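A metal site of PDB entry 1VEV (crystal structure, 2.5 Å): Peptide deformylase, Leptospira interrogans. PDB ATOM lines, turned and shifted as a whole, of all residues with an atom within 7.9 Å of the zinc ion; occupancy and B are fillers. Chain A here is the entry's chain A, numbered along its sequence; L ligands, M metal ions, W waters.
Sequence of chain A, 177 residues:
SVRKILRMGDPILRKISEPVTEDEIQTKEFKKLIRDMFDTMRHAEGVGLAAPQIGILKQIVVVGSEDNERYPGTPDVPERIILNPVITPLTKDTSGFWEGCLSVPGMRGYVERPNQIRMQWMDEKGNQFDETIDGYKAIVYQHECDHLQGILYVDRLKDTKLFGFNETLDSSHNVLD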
ATOM      1  N   ILE A   5     -25.286  38.039  28.504  1.00  0.00           N
ATOM      2  CA  ILE A   5     -25.110  36.676  27.989  1.00  0.00           C
ATOM      3  C   ILE A   5     -23.701  36.218  28.328  1.00  0.00           C
ATOM      4  O   ILE A   5     -22.741  36.646  27.675  1.00  0.00           O
ATOM      5  CB  ILE A   5     -25.251  36.623  26.446  1.00  0.00           C
ATOM      6  CG1 ILE A   5     -26.659  37.069  26.027  1.00  0.00           C
ATOM      7  CG2 ILE A   5     -24.934  35.213  25.946  1.00  0.00           C
ATOM      8  CD1 ILE A   5     -26.876  37.053  24.519  1.00  0.00           C
ATOM      9  N   LEU A  13     -21.700  28.341  32.806  1.00  0.00           N
ATOM     10  CA  LEU A  13     -21.989  27.626  31.569  1.00  0.00           C
ATOM     11  C   LEU A  13     -21.612  26.129  31.564  1.00  0.00           C
ATOM     12  O   LEU A  13     -21.961  25.410  30.625  1.00  0.00           O
ATOM     13  CB  LEU A  13     -21.304  28.322  30.390  1.00  0.00           C
ATOM     14  CG  LEU A  13     -21.788  29.742  30.121  1.00  0.00           C
ATOM     15  CD1 LEU A  13     -21.010  30.348  28.955  1.00  0.00           C
ATOM     16  CD2 LEU A  13     -23.280  29.728  29.813  1.00  0.00           C
ATOM     17  N   GLY A  48     -31.940  30.551  19.586  1.00  0.00           N
ATOM     18  CA  GLY A  48     -32.366  29.953  20.830  1.00  0.00           C
ATOM     19  C   GLY A  48     -31.597  30.566  21.974  1.00  0.00           C
ATOM     20  O   GLY A  48     -30.716  31.402  21.763  1.00  0.00           O
ATOM     21  N   LEU A  49     -31.934  30.190  23.190  1.00  0.00           N
ATOM     22  CA  LEU A  49     -31.249  30.718  24.365  1.00  0.00           C
ATOM     23  C   LEU A  49     -31.662  29.919  25.575  1.00  0.00           C
ATOM     24  O   LEU A  49     -32.842  29.671  25.797  1.00  0.00           O
ATOM     25  CB  LEU A  49     -31.614  32.184  24.563  1.00  0.00           C
ATOM     26  CG  LEU A  49     -30.895  32.878  25.715  1.00  0.00           C
ATOM     27  CD1 LEU A  49     -29.412  33.011  25.368  1.00  0.00           C
ATOM     28  CD2 LEU A  49     -31.498  34.243  25.974  1.00  0.00           C
ATOM     29  N   ALA A  50     -30.693  29.503  26.380  1.00  0.00           N
ATOM     30  CA  ALA A  50     -30.988  28.746  27.582  1.00  0.00           C
ATOM     31  C   ALA A  50     -30.719  29.628  28.792  1.00  0.00           C
ATOM     32  O   ALA A  50     -29.820  30.462  28.783  1.00  0.00           O
ATOM     33  CB  ALA A  50     -30.129  27.499  27.648  1.00  0.00           C
ATOM     34  N   GLN A  53     -27.293  30.538  30.038  1.00  0.00           N
ATOM     35  CA  GLN A  53     -26.557  31.548  29.295  1.00  0.00           C
ATOM     36  C   GLN A  53     -26.690  32.936  29.917  1.00  0.00           C
ATOM     37  O   GLN A  53     -25.772  33.747  29.834  1.00  0.00           O
ATOM     38  CB  GLN A  53     -26.987  31.574  27.828  1.00  0.00           C
ATOM     39  CG  GLN A  53     -26.692  30.277  27.096  1.00  0.00           C
ATOM     40  CD  GLN A  53     -26.944  30.357  25.602  1.00  0.00           C
ATOM     41  OE1 GLN A  53     -26.161  30.931  24.849  1.00  0.00           O
ATOM     42  NE2 GLN A  53     -28.055  29.774  25.164  1.00  0.00           N
ATOM     43  N   ARG A  70     -27.750  36.197  11.338  1.00  0.00           N
ATOM     44  CA  ARG A  70     -26.576  35.414  11.670  1.00  0.00           C
ATOM     45  C   ARG A  70     -26.475  34.080  10.931  1.00  0.00           C
ATOM     46  O   ARG A  70     -25.378  33.649  10.591  1.00  0.00           O
ATOM     47  CB  ARG A  70     -26.514  35.199  13.186  1.00  0.00           C
ATOM     48  CG  ARG A  70     -26.250  36.484  13.967  1.00  0.00           C
ATOM     49  CD  ARG A  70     -26.244  36.248  15.474  1.00  0.00           C
ATOM     50  NE  ARG A  70     -25.351  35.142  15.825  1.00  0.00           N
ATOM     51  CZ  ARG A  70     -25.633  34.228  16.736  1.00  0.00           C
ATOM     52  NH1 ARG A  70     -24.778  33.248  17.000  1.00  0.00           N
ATOM     53  NH2 ARG A  70     -26.787  34.292  17.395  1.00  0.00           N
ATOM     54  N   TYR A  71     -27.599  33.426  10.665  1.00  0.00           N
ATOM     55  CA  TYR A  71     -27.595  32.153   9.937  1.00  0.00           C
ATOM     56  C   TYR A  71     -28.531  32.216   8.736  1.00  0.00           C
ATOM     57  O   TYR A  71     -29.628  31.667   8.776  1.00  0.00           O
ATOM     58  CB  TYR A  71     -28.007  30.995  10.838  1.00  0.00           C
ATOM     59  CG  TYR A  71     -27.177  30.866  12.094  1.00  0.00           C
ATOM     60  CD1 TYR A  71     -27.436  31.655  13.202  1.00  0.00           C
ATOM     61  CD2 TYR A  71     -26.105  29.964  12.154  1.00  0.00           C
ATOM     62  CE1 TYR A  71     -26.666  31.548  14.349  1.00  0.00           C
ATOM     63  CE2 TYR A  71     -25.319  29.860  13.305  1.00  0.00           C
ATOM     64  CZ  TYR A  71     -25.613  30.658  14.403  1.00  0.00           C
ATOM     65  OH  TYR A  71     -24.859  30.585  15.548  1.00  0.00           O
ATOM     66  N   GLU A  99     -22.337  25.424  13.390  1.00  0.00           N
ATOM     67  CA  GLU A  99     -22.971  26.044  14.540  1.00  0.00           C
ATOM     68  C   GLU A  99     -22.201  27.219  15.146  1.00  0.00           C
ATOM     69  O   GLU A  99     -20.984  27.340  14.995  1.00  0.00           O
ATOM     70  CB  GLU A  99     -23.194  24.997  15.630  1.00  0.00           C
ATOM     71  CG  GLU A  99     -24.332  24.049  15.354  1.00  0.00           C
ATOM     72  CD  GLU A  99     -24.529  23.041  16.464  1.00  0.00           C
ATOM     73  OE1 GLU A  99     -24.579  23.444  17.645  1.00  0.00           O
ATOM     74  OE2 GLU A  99     -24.634  21.843  16.140  1.00  0.00           O
ATOM     75  N   GLY A 100     -22.960  28.078  15.830  1.00  0.00           N
ATOM     76  CA  GLY A 100     -22.410  29.225  16.510  1.00  0.00           C
ATOM     77  C   GLY A 100     -23.139  29.289  17.847  1.00  0.00           C
ATOM     78  O   GLY A 100     -24.147  28.623  18.024  1.00  0.00           O
ATOM     79  N   CYS A 101     -22.631  30.069  18.800  1.00  0.00           N
ATOM     80  CA  CYS A 101     -23.288  30.175  20.103  1.00  0.00           C
ATOM     81  C   CYS A 101     -23.110  31.587  20.654  1.00  0.00           C
ATOM     82  O   CYS A 101     -22.023  32.148  20.602  1.00  0.00           O
ATOM     83  CB  CYS A 101     -22.689  29.157  21.079  1.00  0.00           C
ATOM     84  SG  CYS A 101     -23.252  29.324  22.787  1.00  0.00           S
ATOM     85  N   LEU A 102     -24.187  32.165  21.164  1.00  0.00           N
ATOM     86  CA  LEU A 102     -24.134  33.519  21.711  1.00  0.00           C
ATOM     87  C   LEU A 102     -23.177  33.629  22.890  1.00  0.00           C
ATOM     88  O   LEU A 102     -22.824  34.739  23.313  1.00  0.00           O
ATOM     89  CB  LEU A 102     -25.532  33.984  22.124  1.00  0.00           C
ATOM     90  CG  LEU A 102     -26.540  34.128  20.984  1.00  0.00           C
ATOM     91  CD1 LEU A 102     -27.907  34.428  21.568  1.00  0.00           C
ATOM     92  CD2 LEU A 102     -26.103  35.237  20.044  1.00  0.00           C
ATOM     93  N   SER A 103     -22.757  32.494  23.428  1.00  0.00           N
ATOM     94  CA  SER A 103     -21.821  32.506  24.555  1.00  0.00           C
ATOM     95  C   SER A 103     -20.400  32.307  24.016  1.00  0.00           C
ATOM     96  O   SER A 103     -19.433  32.273  24.786  1.00  0.00           O
ATOM     97  CB  SER A 103     -22.152  31.391  25.549  1.00  0.00           C
ATOM     98  OG  SER A 103     -23.379  31.639  26.212  1.00  0.00           O
ATOM     99  N   VAL A 104     -20.291  32.168  22.706  1.00  0.00           N
ATOM    100  CA  VAL A 104     -19.009  31.975  22.038  1.00  0.00           C
ATOM    101  C   VAL A 104     -18.993  32.922  20.852  1.00  0.00           C
ATOM    102  O   VAL A 104     -19.017  32.492  19.704  1.00  0.00           O
ATOM    103  CB  VAL A 104     -18.852  30.532  21.540  1.00  0.00           C
ATOM    104  CG1 VAL A 104     -17.449  30.312  21.026  1.00  0.00           C
ATOM    105  CG2 VAL A 104     -19.184  29.553  22.659  1.00  0.00           C
ATOM    106  N   ARG A 113     -24.834  16.468  14.474  1.00  0.00           N
ATOM    107  CA  ARG A 113     -25.762  15.964  15.489  1.00  0.00           C
ATOM    108  C   ARG A 113     -26.760  15.063  14.759  1.00  0.00           C
ATOM    109  O   ARG A 113     -26.894  15.123  13.545  1.00  0.00           O
ATOM    110  CB  ARG A 113     -26.508  17.115  16.148  1.00  0.00           C
ATOM    111  CG  ARG A 113     -25.630  18.110  16.894  1.00  0.00           C
ATOM    112  CD  ARG A 113     -26.451  19.345  17.303  1.00  0.00           C
ATOM    113  NE  ARG A 113     -25.625  20.383  17.904  1.00  0.00           N
ATOM    114  CZ  ARG A 113     -25.257  20.396  19.180  1.00  0.00           C
ATOM    115  NH1 ARG A 113     -25.652  19.422  20.006  1.00  0.00           N
ATOM    116  NH2 ARG A 113     -24.464  21.365  19.618  1.00  0.00           N
ATOM    117  N   VAL A 140     -31.180  22.820  16.676  1.00  0.00           N
ATOM    118  CA  VAL A 140     -31.344  23.883  17.655  1.00  0.00           C
ATOM    119  C   VAL A 140     -31.678  23.331  19.038  1.00  0.00           C
ATOM    120  O   VAL A 140     -31.065  23.698  20.040  1.00  0.00           O
ATOM    121  CB  VAL A 140     -32.470  24.881  17.255  1.00  0.00           C
ATOM    122  CG1 VAL A 140     -32.669  25.911  18.364  1.00  0.00           C
ATOM    123  CG2 VAL A 140     -32.104  25.591  15.960  1.00  0.00           C
ATOM    124  N   HIS A 143     -28.765  21.552  20.626  1.00  0.00           N
ATOM    125  CA  HIS A 143     -27.803  22.572  21.009  1.00  0.00           C
ATOM    126  C   HIS A 143     -28.250  23.263  22.292  1.00  0.00           C
ATOM    127  O   HIS A 143     -27.437  23.525  23.183  1.00  0.00           O
ATOM    128  CB  HIS A 143     -27.674  23.599  19.877  1.00  0.00           C
ATOM    129  CG  HIS A 143     -26.804  24.763  20.220  1.00  0.00           C
ATOM    130  ND1 HIS A 143     -25.508  24.912  19.780  1.00  0.00           N
ATOM    131  CD2 HIS A 143     -27.056  25.841  21.004  1.00  0.00           C
ATOM    132  CE1 HIS A 143     -25.031  26.057  20.301  1.00  0.00           C
ATOM    133  NE2 HIS A 143     -25.935  26.653  21.052  1.00  0.00           N
ATOM    134  N   GLU A 144     -29.535  23.552  22.393  1.00  0.00           N
ATOM    135  CA  GLU A 144     -30.035  24.211  23.588  1.00  0.00           C
ATOM    136  C   GLU A 144     -30.055  23.323  24.823  1.00  0.00           C
ATOM    137  O   GLU A 144     -29.765  23.781  25.924  1.00  0.00           O
ATOM    138  CB  GLU A 144     -31.432  24.782  23.340  1.00  0.00           C
ATOM    139  CG  GLU A 144     -31.532  25.731  22.152  1.00  0.00           C
ATOM    140  CD  GLU A 144     -30.481  26.840  22.167  1.00  0.00           C
ATOM    141  OE1 GLU A 144     -30.117  27.305  23.266  1.00  0.00           O
ATOM    142  OE2 GLU A 144     -30.036  27.249  21.078  1.00  0.00           O
ATOM    143  N   ASP A 146     -28.018  20.890  25.534  1.00  0.00           N
ATOM    144  CA  ASP A 146     -26.650  20.706  25.991  1.00  0.00           C
ATOM    145  C   ASP A 146     -26.349  21.768  27.045  1.00  0.00           C
ATOM    146  O   ASP A 146     -25.765  21.471  28.083  1.00  0.00           O
ATOM    147  CB  ASP A 146     -25.676  20.828  24.807  1.00  0.00           C
ATOM    148  CG  ASP A 146     -25.598  19.549  23.961  1.00  0.00           C
ATOM    149  OD1 ASP A 146     -25.126  19.616  22.810  1.00  0.00           O
ATOM    150  OD2 ASP A 146     -25.983  18.465  24.463  1.00  0.00           O
ATOM    151  N   HIS A 147     -26.784  23.002  26.790  1.00  0.00           N
ATOM    152  CA  HIS A 147     -26.583  24.103  27.735  1.00  0.00           C
ATOM    153  C   HIS A 147     -27.106  23.773  29.124  1.00  0.00           C
ATOM    154  O   HIS A 147     -26.474  24.114  30.133  1.00  0.00           O
ATOM    155  CB  HIS A 147     -27.294  25.365  27.258  1.00  0.00           C
ATOM    156  CG  HIS A 147     -26.517  26.159  26.255  1.00  0.00           C
ATOM    157  ND1 HIS A 147     -25.285  26.724  26.504  1.00  0.00           N
ATOM    158  CD2 HIS A 147     -26.836  26.537  24.994  1.00  0.00           C
ATOM    159  CE1 HIS A 147     -24.924  27.417  25.430  1.00  0.00           C
ATOM    160  NE2 HIS A 147     -25.841  27.340  24.485  1.00  0.00           N
ATOM    161  N   ILE A 151     -22.987  21.805  28.606  1.00  0.00           N
ATOM    162  CA  ILE A 151     -22.248  21.442  27.401  1.00  0.00           C
ATOM    163  C   ILE A 151     -22.378  22.530  26.334  1.00  0.00           C
ATOM    164  O   ILE A 151     -23.475  23.027  26.091  1.00  0.00           O
ATOM    165  CB  ILE A 151     -22.792  20.131  26.829  1.00  0.00           C
ATOM    166  CG1 ILE A 151     -22.640  19.008  27.858  1.00  0.00           C
ATOM    167  CG2 ILE A 151     -22.082  19.795  25.509  1.00  0.00           C
ATOM    168  CD1 ILE A 151     -23.266  17.696  27.439  1.00  0.00           C
ATOM    169  N   LEU A 152     -21.263  22.905  25.713  1.00  0.00           N
ATOM    170  CA  LEU A 152     -21.259  23.909  24.663  1.00  0.00           C
ATOM    171  C   LEU A 152     -20.887  23.207  23.348  1.00  0.00           C
ATOM    172  O   LEU A 152     -20.298  22.120  23.374  1.00  0.00           O
ATOM    173  CB  LEU A 152     -20.253  25.016  24.981  1.00  0.00           C
ATOM    174  CG  LEU A 152     -20.564  25.822  26.253  1.00  0.00           C
ATOM    175  CD1 LEU A 152     -19.434  26.805  26.538  1.00  0.00           C
ATOM    176  CD2 LEU A 152     -21.886  26.562  26.084  1.00  0.00           C
ATOM    177  N   TYR A 153     -21.225  23.804  22.214  1.00  0.00           N
ATOM    178  CA  TYR A 153     -20.957  23.164  20.934  1.00  0.00           C
ATOM    179  C   TYR A 153     -19.479  22.879  20.641  1.00  0.00           C
ATOM    180  O   TYR A 153     -19.153  21.988  19.854  1.00  0.00           O
ATOM    181  CB  TYR A 153     -21.578  23.979  19.797  1.00  0.00           C
ATOM    182  CG  TYR A 153     -20.735  25.121  19.286  1.00  0.00           C
ATOM    183  CD1 TYR A 153     -19.800  24.919  18.267  1.00  0.00           C
ATOM    184  CD2 TYR A 153     -20.890  26.408  19.805  1.00  0.00           C
ATOM    185  CE1 TYR A 153     -19.041  25.975  17.787  1.00  0.00           C
ATOM    186  CE2 TYR A 153     -20.136  27.470  19.319  1.00  0.00           C
ATOM    187  CZ  TYR A 153     -19.219  27.246  18.308  1.00  0.00           C
ATOM    188  OH  TYR A 153     -18.471  28.294  17.829  1.00  0.00           O
HETATM  189  C1  LIG L   1     -27.864  30.234  22.183  1.00  0.00           C
HETATM  190  O1  LIG L   1     -26.775  30.371  21.688  1.00  0.00           O
HETATM  191  O2  LIG L   1     -28.542  29.108  22.270  1.00  0.00           O
HETATM  192 ZN    ZN M   1     -25.804  28.282  22.639  1.00  0.00          ZN
HETATM  193  O   HOH W   1     -23.002  26.253  22.788  1.00  0.00           O
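OE1 of Gln 53 touches the zinc ion, at 3.5 Å.
Four residues have an atom within 4 Å of the zinc ion: Gln 53, Cys 101, His 143 and His 147.
The nearest printed residue that does not touch the zinc ion is Leu 102 (4.5 Å).
The zinc ion is bound by a ring nitrogen (NE2) of His 147 (2.1 Å), a ring nitrogen (NE2) of His 143 (2.3 Å), an oxygen (O1) of the ligand (2.5 Å) and the side-chain sulfur of Cys 101 (2.8 Å).
The side-chain amide nitrogen (NE2) of Gln 53 lies close to the backbone NH (N) of Ala 50, 2.9 Å away.
The side-chain amide oxygen (OE1) of Gln 53 is in hydrogen-bond range of the side-chain hydroxyl (OG) of Ser 103 (3.2 Å).
A ring nitrogen (NE2) of His 147 lies close to the side-chain amide nitrogen (NE2) of Gln 53 (3.4 Å).
The side-chain carboxylate (OE1) of Glu 99 lies within hydrogen-bond range of a ring nitrogen (ND1) of His 143.
The side-chain sulfur of Cys 101 sits close to the backbone NH of Ser 103, 3.3 Å away.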
